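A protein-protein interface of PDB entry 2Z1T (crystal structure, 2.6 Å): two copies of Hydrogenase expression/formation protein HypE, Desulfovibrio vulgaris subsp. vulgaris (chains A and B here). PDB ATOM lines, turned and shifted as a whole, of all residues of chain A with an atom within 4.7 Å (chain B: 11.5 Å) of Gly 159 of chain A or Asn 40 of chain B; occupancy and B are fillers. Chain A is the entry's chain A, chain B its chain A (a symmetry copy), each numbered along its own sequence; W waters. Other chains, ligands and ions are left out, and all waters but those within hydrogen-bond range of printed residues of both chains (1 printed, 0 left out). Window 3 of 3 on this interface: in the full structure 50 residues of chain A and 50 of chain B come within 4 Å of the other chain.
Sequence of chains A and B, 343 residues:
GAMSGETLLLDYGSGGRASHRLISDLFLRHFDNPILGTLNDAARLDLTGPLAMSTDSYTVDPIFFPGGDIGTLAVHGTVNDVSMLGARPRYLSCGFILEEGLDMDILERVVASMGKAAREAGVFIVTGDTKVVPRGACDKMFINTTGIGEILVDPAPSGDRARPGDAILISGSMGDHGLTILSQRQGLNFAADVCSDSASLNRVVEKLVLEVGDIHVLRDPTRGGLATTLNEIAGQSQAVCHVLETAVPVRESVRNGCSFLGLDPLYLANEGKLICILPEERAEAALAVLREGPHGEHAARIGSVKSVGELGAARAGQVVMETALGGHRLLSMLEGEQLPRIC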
ATOM      1  N   LEU A  85     -11.754  16.535  12.424  1.00  0.00           N
ATOM      2  CA  LEU A  85     -10.558  15.712  12.487  1.00  0.00           C
ATOM      3  C   LEU A  85     -10.538  14.840  13.765  1.00  0.00           C
ATOM      4  O   LEU A  85      -9.481  14.385  14.215  1.00  0.00           O
ATOM      5  CB  LEU A  85      -9.313  16.597  12.379  1.00  0.00           C
ATOM      6  CG  LEU A  85      -8.337  16.117  11.306  1.00  0.00           C
ATOM      7  CD1 LEU A  85      -8.982  16.248   9.928  1.00  0.00           C
ATOM      8  CD2 LEU A  85      -7.002  16.860  11.338  1.00  0.00           C
ATOM      9  N   PRO A 157     -10.372  10.683  11.898  1.00  0.00           N
ATOM     10  CA  PRO A 157     -11.300  10.698  10.758  1.00  0.00           C
ATOM     11  C   PRO A 157     -10.747  11.531   9.614  1.00  0.00           C
ATOM     12  O   PRO A 157     -10.085  12.542   9.849  1.00  0.00           O
ATOM     13  CB  PRO A 157     -12.563  11.342  11.334  1.00  0.00           C
ATOM     14  CG  PRO A 157     -12.468  11.122  12.806  1.00  0.00           C
ATOM     15  CD  PRO A 157     -11.009  11.208  13.120  1.00  0.00           C
ATOM     16  N   SER A 158     -10.984  11.086   8.383  1.00  0.00           N
ATOM     17  CA  SER A 158     -10.420  11.749   7.219  1.00  0.00           C
ATOM     18  C   SER A 158     -11.148  11.334   5.949  1.00  0.00           C
ATOM     19  O   SER A 158     -11.340  10.145   5.684  1.00  0.00           O
ATOM     20  CB  SER A 158      -8.922  11.449   7.108  1.00  0.00           C
ATOM     21  OG  SER A 158      -8.439  11.771   5.822  1.00  0.00           O
ATOM     22  N   GLY A 159     -11.520  12.323   5.152  1.00  0.00           N
ATOM     23  CA  GLY A 159     -12.269  12.111   3.920  1.00  0.00           C
ATOM     24  C   GLY A 159     -11.830  10.973   3.028  1.00  0.00           C
ATOM     25  O   GLY A 159     -12.586  10.562   2.152  1.00  0.00           O
ATOM     26  N   ASP A 160     -10.624  10.452   3.243  1.00  0.00           N
ATOM     27  CA  ASP A 160     -10.102   9.351   2.409  1.00  0.00           C
ATOM     28  C   ASP A 160     -10.162   7.990   3.105  1.00  0.00           C
ATOM     29  O   ASP A 160      -9.562   7.029   2.639  1.00  0.00           O
ATOM     30  CB  ASP A 160      -8.664   9.646   1.935  1.00  0.00           C
ATOM     31  CG  ASP A 160      -7.641   9.713   3.092  1.00  0.00           C
ATOM     32  OD1 ASP A 160      -8.019   9.795   4.286  1.00  0.00           O
ATOM     33  OD2 ASP A 160      -6.434   9.689   2.786  1.00  0.00           O
ATOM     34  N   ARG A 161     -10.876   7.917   4.222  1.00  0.00           N
ATOM     35  CA  ARG A 161     -10.888   6.709   5.039  1.00  0.00           C
ATOM     36  C   ARG A 161     -12.210   5.956   5.017  1.00  0.00           C
ATOM     37  O   ARG A 161     -12.396   5.006   5.782  1.00  0.00           O
ATOM     38  CB  ARG A 161     -10.481   7.033   6.477  1.00  0.00           C
ATOM     39  CG  ARG A 161      -8.984   7.221   6.627  1.00  0.00           C
ATOM     40  CD  ARG A 161      -8.530   7.242   8.077  1.00  0.00           C
ATOM     41  NE  ARG A 161      -8.824   5.995   8.790  1.00  0.00           N
ATOM     42  CZ  ARG A 161      -9.660   5.901   9.825  1.00  0.00           C
ATOM     43  NH1 ARG A 161     -10.294   6.979  10.277  1.00  0.00           N
ATOM     44  NH2 ARG A 161      -9.865   4.727  10.415  1.00  0.00           N
ATOM     45  N   ALA A 162     -13.129   6.387   4.153  1.00  0.00           N
ATOM     46  CA  ALA A 162     -14.374   5.651   3.930  1.00  0.00           C
ATOM     47  C   ALA A 162     -13.979   4.363   3.243  1.00  0.00           C
ATOM     48  O   ALA A 162     -13.077   4.363   2.391  1.00  0.00           O
ATOM     49  CB  ALA A 162     -15.340   6.444   3.080  1.00  0.00           C
ATOM     50  N   VAL A 217     -14.862   8.546   8.849  1.00  0.00           N
ATOM     51  CA  VAL A 217     -14.991   9.874   8.257  1.00  0.00           C
ATOM     52  C   VAL A 217     -15.997  10.717   9.035  1.00  0.00           C
ATOM     53  O   VAL A 217     -17.112  10.259   9.333  1.00  0.00           O
ATOM     54  CB  VAL A 217     -15.441   9.807   6.792  1.00  0.00           C
ATOM     55  CG1 VAL A 217     -15.503  11.206   6.185  1.00  0.00           C
ATOM     56  CG2 VAL A 217     -14.515   8.919   5.977  1.00  0.00           C
ATOM     57  N   ARG A 219     -17.493  14.800   8.700  1.00  0.00           N
ATOM     58  CA  ARG A 219     -17.553  15.904   7.785  1.00  0.00           C
ATOM     59  C   ARG A 219     -18.873  16.606   8.007  1.00  0.00           C
ATOM     60  O   ARG A 219     -19.859  15.952   8.341  1.00  0.00           O
ATOM     61  CB  ARG A 219     -17.498  15.351   6.363  1.00  0.00           C
ATOM     62  CG  ARG A 219     -16.845  16.231   5.370  1.00  0.00           C
ATOM     63  CD  ARG A 219     -15.321  16.305   5.549  1.00  0.00           C
ATOM     64  NE  ARG A 219     -14.652  16.086   4.286  1.00  0.00           N
ATOM     65  CZ  ARG A 219     -14.918  16.782   3.184  1.00  0.00           C
ATOM     66  NH1 ARG A 219     -15.825  17.770   3.233  1.00  0.00           N
ATOM     67  NH2 ARG A 219     -14.279  16.490   2.043  1.00  0.00           N
ATOM     68  N   ILE A 233     -16.106  13.003  -0.345  1.00  0.00           N
ATOM     69  CA  ILE A 233     -15.714  11.786   0.368  1.00  0.00           C
ATOM     70  C   ILE A 233     -15.565  10.616  -0.602  1.00  0.00           C
ATOM     71  O   ILE A 233     -14.516   9.976  -0.650  1.00  0.00           O
ATOM     72  CB  ILE A 233     -16.730  11.388   1.462  1.00  0.00           C
ATOM     73  CG1 ILE A 233     -16.809  12.464   2.552  1.00  0.00           C
ATOM     74  CG2 ILE A 233     -16.360  10.021   2.061  1.00  0.00           C
ATOM     75  CD1 ILE A 233     -18.091  12.452   3.360  1.00  0.00           C
ATOM     76  N   GLN A 236     -12.384  11.177  -2.526  1.00  0.00           N
ATOM     77  CA  GLN A 236     -11.161  10.980  -1.759  1.00  0.00           C
ATOM     78  C   GLN A 236     -10.909   9.547  -1.358  1.00  0.00           C
ATOM     79  O   GLN A 236      -9.766   9.125  -1.283  1.00  0.00           O
ATOM     80  CB  GLN A 236     -11.157  11.874  -0.525  1.00  0.00           C
ATOM     81  CG  GLN A 236     -10.639  13.249  -0.821  1.00  0.00           C
ATOM     82  CD  GLN A 236     -11.288  14.336   0.016  1.00  0.00           C
ATOM     83  OE1 GLN A 236     -11.858  15.280  -0.540  1.00  0.00           O
ATOM     84  NE2 GLN A 236     -11.194  14.229   1.356  1.00  0.00           N
ATOM     85  N   SER A 237     -11.965   8.789  -1.108  1.00  0.00           N
ATOM     86  CA  SER A 237     -11.805   7.402  -0.667  1.00  0.00           C
ATOM     87  C   SER A 237     -11.721   6.421  -1.822  1.00  0.00           C
ATOM     88  O   SER A 237     -11.210   5.316  -1.664  1.00  0.00           O
ATOM     89  CB  SER A 237     -12.910   7.014   0.317  1.00  0.00           C
ATOM     90  OG  SER A 237     -12.946   7.942   1.396  1.00  0.00           O
ATOM     91  N   ASP B  25      -7.766  26.952  -8.125  1.00  0.00           N
ATOM     92  CA  ASP B  25      -6.744  26.074  -7.543  1.00  0.00           C
ATOM     93  C   ASP B  25      -5.324  26.214  -8.134  1.00  0.00           C
ATOM     94  O   ASP B  25      -4.636  25.249  -8.489  1.00  0.00           O
ATOM     95  CB  ASP B  25      -7.259  24.651  -7.401  1.00  0.00           C
ATOM     96  CG  ASP B  25      -8.070  24.489  -6.140  1.00  0.00           C
ATOM     97  OD1 ASP B  25      -7.458  24.488  -5.055  1.00  0.00           O
ATOM     98  OD2 ASP B  25      -9.312  24.407  -6.220  1.00  0.00           O
ATOM     99  N   ASN B  33       1.741  21.245  -0.450  1.00  0.00           N
ATOM    100  CA  ASN B  33       2.381  20.400   0.556  1.00  0.00           C
ATOM    101  C   ASN B  33       1.344  19.362   0.996  1.00  0.00           C
ATOM    102  O   ASN B  33       0.139  19.590   0.805  1.00  0.00           O
ATOM    103  CB  ASN B  33       2.870  21.226   1.751  1.00  0.00           C
ATOM    104  CG  ASN B  33       1.737  21.934   2.479  1.00  0.00           C
ATOM    105  OD1 ASN B  33       1.180  21.406   3.447  1.00  0.00           O
ATOM    106  ND2 ASN B  33       1.379  23.126   2.003  1.00  0.00           N
ATOM    107  N   PRO B  34       1.786  18.227   1.588  1.00  0.00           N
ATOM    108  CA  PRO B  34       0.842  17.117   1.854  1.00  0.00           C
ATOM    109  C   PRO B  34      -0.181  17.403   2.968  1.00  0.00           C
ATOM    110  O   PRO B  34      -1.218  16.733   3.025  1.00  0.00           O
ATOM    111  CB  PRO B  34       1.765  15.960   2.249  1.00  0.00           C
ATOM    112  CG  PRO B  34       2.979  16.641   2.840  1.00  0.00           C
ATOM    113  CD  PRO B  34       3.157  17.914   2.052  1.00  0.00           C
ATOM    114  N   ILE B  35       0.117  18.386   3.830  1.00  0.00           N
ATOM    115  CA  ILE B  35      -0.815  18.858   4.880  1.00  0.00           C
ATOM    116  C   ILE B  35      -2.010  19.637   4.291  1.00  0.00           C
ATOM    117  O   ILE B  35      -3.157  19.411   4.688  1.00  0.00           O
ATOM    118  CB  ILE B  35      -0.106  19.713   5.988  1.00  0.00           C
ATOM    119  CG1 ILE B  35       1.134  18.999   6.543  1.00  0.00           C
ATOM    120  CG2 ILE B  35      -1.065  20.029   7.131  1.00  0.00           C
ATOM    121  CD1 ILE B  35       2.108  19.912   7.302  1.00  0.00           C
ATOM    122  N   LEU B  36      -1.736  20.544   3.348  1.00  0.00           N
ATOM    123  CA  LEU B  36      -2.794  21.246   2.595  1.00  0.00           C
ATOM    124  C   LEU B  36      -3.486  20.340   1.554  1.00  0.00           C
ATOM    125  O   LEU B  36      -4.710  20.410   1.385  1.00  0.00           O
ATOM    126  CB  LEU B  36      -2.245  22.520   1.924  1.00  0.00           C
ATOM    127  CG  LEU B  36      -3.184  23.380   1.063  1.00  0.00           C
ATOM    128  CD1 LEU B  36      -3.984  24.389   1.890  1.00  0.00           C
ATOM    129  CD2 LEU B  36      -2.404  24.091  -0.031  1.00  0.00           C
ATOM    130  N   GLY B  37      -2.700  19.493   0.882  1.00  0.00           N
ATOM    131  CA  GLY B  37      -3.181  18.671  -0.235  1.00  0.00           C
ATOM    132  C   GLY B  37      -3.895  17.397   0.188  1.00  0.00           C
ATOM    133  O   GLY B  37      -3.942  16.410  -0.563  1.00  0.00           O
ATOM    134  N   THR B  38      -4.440  17.432   1.400  1.00  0.00           N
ATOM    135  CA  THR B  38      -5.250  16.352   1.951  1.00  0.00           C
ATOM    136  C   THR B  38      -6.732  16.787   1.919  1.00  0.00           C
ATOM    137  O   THR B  38      -7.645  15.949   1.909  1.00  0.00           O
ATOM    138  CB  THR B  38      -4.760  15.989   3.380  1.00  0.00           C
ATOM    139  OG1 THR B  38      -4.857  14.573   3.575  1.00  0.00           O
ATOM    140  CG2 THR B  38      -5.542  16.743   4.470  1.00  0.00           C
ATOM    141  N   LEU B  39      -6.925  18.111   1.921  1.00  0.00           N
ATOM    142  CA  LEU B  39      -8.198  18.793   1.645  1.00  0.00           C
ATOM    143  C   LEU B  39      -9.441  18.351   2.437  1.00  0.00           C
ATOM    144  O   LEU B  39     -10.516  18.118   1.869  1.00  0.00           O
ATOM    145  CB  LEU B  39      -8.458  18.900   0.122  1.00  0.00           C
ATOM    146  CG  LEU B  39      -7.797  20.126  -0.555  1.00  0.00           C
ATOM    147  CD1 LEU B  39      -8.041  20.195  -2.071  1.00  0.00           C
ATOM    148  CD2 LEU B  39      -8.213  21.466   0.120  1.00  0.00           C
ATOM    149  N   ASN B  40      -9.246  18.263   3.757  1.00  0.00           N
ATOM    150  CA  ASN B  40     -10.289  18.051   4.772  1.00  0.00           C
ATOM    151  C   ASN B  40     -10.781  19.372   5.391  1.00  0.00           C
ATOM    152  O   ASN B  40     -10.194  20.455   5.151  1.00  0.00           O
ATOM    153  CB  ASN B  40      -9.715  17.207   5.914  1.00  0.00           C
ATOM    154  CG  ASN B  40      -9.777  15.728   5.647  1.00  0.00           C
ATOM    155  OD1 ASN B  40     -10.693  15.237   4.988  1.00  0.00           O
ATOM    156  ND2 ASN B  40      -8.809  14.993   6.187  1.00  0.00           N
ATOM    157  N   ASP B  41     -11.820  19.263   6.230  1.00  0.00           N
ATOM    158  CA  ASP B  41     -12.318  20.394   7.052  1.00  0.00           C
ATOM    159  C   ASP B  41     -11.259  21.088   7.924  1.00  0.00           C
ATOM    160  O   ASP B  41     -11.369  22.292   8.189  1.00  0.00           O
ATOM    161  CB  ASP B  41     -13.517  19.972   7.921  1.00  0.00           C
ATOM    162  CG  ASP B  41     -14.848  19.960   7.140  1.00  0.00           C
ATOM    163  OD1 ASP B  41     -15.702  19.089   7.427  1.00  0.00           O
ATOM    164  OD2 ASP B  41     -15.042  20.826   6.251  1.00  0.00           O
ATOM    165  N   ALA B  42     -10.246  20.335   8.352  1.00  0.00           N
ATOM    166  CA  ALA B  42      -9.122  20.884   9.116  1.00  0.00           C
ATOM    167  C   ALA B  42      -7.802  20.225   8.725  1.00  0.00           C
ATOM    168  O   ALA B  42      -7.788  19.093   8.246  1.00  0.00           O
ATOM    169  CB  ALA B  42      -9.373  20.711  10.616  1.00  0.00           C
ATOM    170  N   ALA B  43      -6.696  20.923   8.962  1.00  0.00           N
ATOM    171  CA  ALA B  43      -5.359  20.386   8.717  1.00  0.00           C
ATOM    172  C   ALA B  43      -4.715  19.857   9.990  1.00  0.00           C
ATOM    173  O   ALA B  43      -4.867  20.438  11.038  1.00  0.00           O
ATOM    174  CB  ALA B  43      -4.481  21.432   8.077  1.00  0.00           C
ATOM    175  N   ARG B  44      -4.004  18.744   9.890  1.00  0.00           N
ATOM    176  CA  ARG B  44      -3.306  18.161  11.028  1.00  0.00           C
ATOM    177  C   ARG B  44      -1.918  18.747  11.148  1.00  0.00           C
ATOM    178  O   ARG B  44      -1.201  18.881  10.159  1.00  0.00           O
ATOM    179  CB  ARG B  44      -3.207  16.640  10.916  1.00  0.00           C
ATOM    180  CG  ARG B  44      -2.353  16.003  12.004  1.00  0.00           C
ATOM    181  CD  ARG B  44      -2.074  14.547  11.695  1.00  0.00           C
ATOM    182  NE  ARG B  44      -1.035  13.985  12.562  1.00  0.00           N
ATOM    183  CZ  ARG B  44      -1.204  12.937  13.371  1.00  0.00           C
ATOM    184  NH1 ARG B  44      -2.381  12.306  13.435  1.00  0.00           N
ATOM    185  NH2 ARG B  44      -0.179  12.512  14.110  1.00  0.00           N
ATOM    186  N   LEU B  45      -1.544  19.068  12.378  1.00  0.00           N
ATOM    187  CA  LEU B  45      -0.309  19.764  12.670  1.00  0.00           C
ATOM    188  C   LEU B  45       0.407  18.994  13.748  1.00  0.00           C
ATOM    189  O   LEU B  45      -0.222  18.553  14.702  1.00  0.00           O
ATOM    190  CB  LEU B  45      -0.638  21.150  13.218  1.00  0.00           C
ATOM    191  CG  LEU B  45      -0.681  22.388  12.328  1.00  0.00           C
ATOM    192  CD1 LEU B  45      -1.320  22.165  10.973  1.00  0.00           C
ATOM    193  CD2 LEU B  45      -1.388  23.492  13.065  1.00  0.00           C
ATOM    194  N   SER B  93      -2.619  29.523   8.184  1.00  0.00           N
ATOM    195  CA  SER B  93      -3.880  29.220   7.522  1.00  0.00           C
ATOM    196  C   SER B  93      -4.395  30.454   6.720  1.00  0.00           C
ATOM    197  O   SER B  93      -3.884  31.544   7.067  1.00  0.00           O
ATOM    198  CB  SER B  93      -4.944  28.843   8.556  1.00  0.00           C
ATOM    199  OG  SER B  93      -5.248  29.941   9.399  1.00  0.00           O
ATOM    200  N   CYS B  94      -5.236  30.335   5.740  1.00  0.00           N
ATOM    201  CA  CYS B  94      -5.507  31.569   5.092  1.00  0.00           C
ATOM    202  C   CYS B  94      -6.906  31.649   4.474  1.00  0.00           C
ATOM    203  O   CYS B  94      -7.446  30.658   4.001  1.00  0.00           O
ATOM    204  CB  CYS B  94      -4.420  31.997   4.108  1.00  0.00           C
ATOM    205  SG  CYS B  94      -4.861  31.717   2.439  1.00  0.00           S
ATOM    206  N   ILE B 125       1.573  27.254   4.386  1.00  0.00           N
ATOM    207  CA  ILE B 125       0.132  27.488   4.390  1.00  0.00           C
ATOM    208  C   ILE B 125      -0.561  26.132   4.325  1.00  0.00           C
ATOM    209  O   ILE B 125      -0.525  25.463   3.304  1.00  0.00           O
ATOM    210  CB  ILE B 125      -0.319  28.407   3.243  1.00  0.00           C
ATOM    211  CG1 ILE B 125       0.281  29.800   3.444  1.00  0.00           C
ATOM    212  CG2 ILE B 125      -1.835  28.519   3.226  1.00  0.00           C
ATOM    213  CD1 ILE B 125       0.525  30.573   2.176  1.00  0.00           C
ATOM    214  N   VAL B 126      -1.174  25.718   5.429  1.00  0.00           N
ATOM    215  CA  VAL B 126      -1.644  24.341   5.566  1.00  0.00           C
ATOM    216  C   VAL B 126      -3.136  24.143   5.354  1.00  0.00           C
ATOM    217  O   VAL B 126      -3.571  23.019   5.085  1.00  0.00           O
ATOM    218  CB  VAL B 126      -1.271  23.726   6.941  1.00  0.00           C
ATOM    219  CG1 VAL B 126       0.227  23.642   7.102  1.00  0.00           C
ATOM    220  CG2 VAL B 126      -1.902  24.491   8.066  1.00  0.00           C
ATOM    221  N   THR B 127      -3.917  25.210   5.492  1.00  0.00           N
ATOM    222  CA  THR B 127      -5.361  25.128   5.338  1.00  0.00           C
ATOM    223  C   THR B 127      -5.891  26.490   4.903  1.00  0.00           C
ATOM    224  O   THR B 127      -5.204  27.509   5.068  1.00  0.00           O
ATOM    225  CB  THR B 127      -6.045  24.615   6.639  1.00  0.00           C
ATOM    226  OG1 THR B 127      -7.464  24.538   6.462  1.00  0.00           O
ATOM    227  CG2 THR B 127      -5.750  25.530   7.808  1.00  0.00           C
ATOM    228  N   GLY B 128      -7.093  26.512   4.330  1.00  0.00           N
ATOM    229  CA  GLY B 128      -7.654  27.752   3.836  1.00  0.00           C
ATOM    230  C   GLY B 128      -9.157  27.771   3.759  1.00  0.00           C
ATOM    231  O   GLY B 128      -9.822  26.827   4.164  1.00  0.00           O
ATOM    232  N   ASP B 129      -9.692  28.872   3.250  1.00  0.00           N
ATOM    233  CA  ASP B 129     -11.094  28.986   2.903  1.00  0.00           C
ATOM    234  C   ASP B 129     -11.116  29.992   1.781  1.00  0.00           C
ATOM    235  O   ASP B 129     -10.138  30.712   1.598  1.00  0.00           O
ATOM    236  CB  ASP B 129     -11.913  29.523   4.066  1.00  0.00           C
ATOM    237  CG  ASP B 129     -13.411  29.408   3.830  1.00  0.00           C
ATOM    238  OD1 ASP B 129     -13.851  28.357   3.332  1.00  0.00           O
ATOM    239  OD2 ASP B 129     -14.162  30.345   4.168  1.00  0.00           O
ATOM    240  N   THR B 130     -12.219  30.056   1.034  1.00  0.00           N
ATOM    241  CA  THR B 130     -12.386  31.087   0.008  1.00  0.00           C
ATOM    242  C   THR B 130     -13.863  31.433  -0.136  1.00  0.00           C
ATOM    243  O   THR B 130     -14.676  30.581  -0.500  1.00  0.00           O
ATOM    244  CB  THR B 130     -11.829  30.622  -1.341  1.00  0.00           C
ATOM    245  OG1 THR B 130     -10.505  30.106  -1.157  1.00  0.00           O
ATOM    246  CG2 THR B 130     -11.782  31.763  -2.323  1.00  0.00           C
HETATM  247  O   HOH W   1     -13.530  19.826   1.603  1.00  0.00           O
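Of the printed residues of chain B, Leu 85 of chain A touches Asn 40, Ala 42 and Arg 44.
Ser 158 of chain A touches just one residue of chain B: Asn 40 (3.3 Å).
Gly 159 of chain A touches just one residue of chain B: Asn 40.
No residue of chain B comes within 4 Å of Asp 160 of chain A.
No residue of chain B comes within 4 Å of Ala 162 of chain A.
No residue of chain B comes within 4 Å of Val 217 of chain A.
Of the printed residues of chain B, Arg 219 of chain A touches Asp 41 (3.4 Å).
No residue of chain B comes within 4 Å of Ile 233 of chain A.
Of the printed residues of chain B, Gln 236 of chain A touches Thr 38 (3.98 Å), Leu 39 (3.96 Å) and Asn 40 (3.8 Å).
Pro 34 of chain B touches none of the printed residues of chain A.
Of chain A, only Leu 85 (3.9 Å), Ser 158 (3.3 Å), Gly 159 (3.0 Å) and Gln 236 (3.8 Å) come within 4 Å of Asn 40 of chain B.
Of the printed residues of chain A, Ala 42 of chain B touches Leu 85.
The nearest residue of chain B that does not touch Gly 159 of chain A is Thr 38 of chain B (6.2 Å).
The nearest printed residue of chain B that does not touch Arg 219 of chain A is Leu 39 of chain B (4.1 Å).
Leu 85 of chain A touches Asn 40 of chain B.
Ala 42 of chain B touches Leu 85 of chain A (O to CD1, 3.5 Å).
Arg 44 of chain B touches Leu 85 of chain A (CB to CD2, 3.8 Å).
Arg 219 of chain A touches Asp 41 of chain B (CD to OD1, 3.4 Å).
Gln 236 of chain A touches Thr 38 of chain B (NE2 to O, 3.98 Å).
Gln 236 of chain A touches Leu 39 of chain B (OE1 to O, 3.96 Å).
NE2 of Gln 236 of chain A touches OD1 of Asn 40 of chain B (3.8 Å).
No position is printed for both chains.
Water W1 lies within hydrogen-bond range of the guanidinium group of Arg 219 of chain A (3.4 Å) and the backbone carbonyl oxygen of Leu 39 of chain B (3.5 Å).
The side-chain amide nitrogen of Asn 40 of chain B sits at hydrogen-bond distance from the side-chain hydroxyl of Ser 158 of chain A (3.3 Å).
N of Gly 159 of chain A sits at hydrogen-bond distance from OD1 of Asn 40 of chain B, at 3.0 Å.
Of the 12 printed residues of chain A, 5 touch a printed residue of chain B.
Printed residues of chain A that touch a printed residue of chain B: Leu 85, Ser 158, Gly 159, Arg 219 and Gln 236.
Of the 22 printed residues of chain B, 6 touch a printed residue of chain A.
Among the printed residues, 9 pairs touch across the chains.
Among the printed residues, no Asp or Glu carboxylate lies within 4 Å of a Lys or Arg side-chain nitrogen of the other chain.
OG of Ser 158 of chain A lies within hydrogen-bond range of OD1 of Asp 160 of chain A (2.5 Å).
The backbone carbonyl oxygen (O) of Gly 159 of chain A sits at hydrogen-bond distance from the side-chain hydroxyl (OG) of Ser 237 of chain A, 2.8 Å away.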
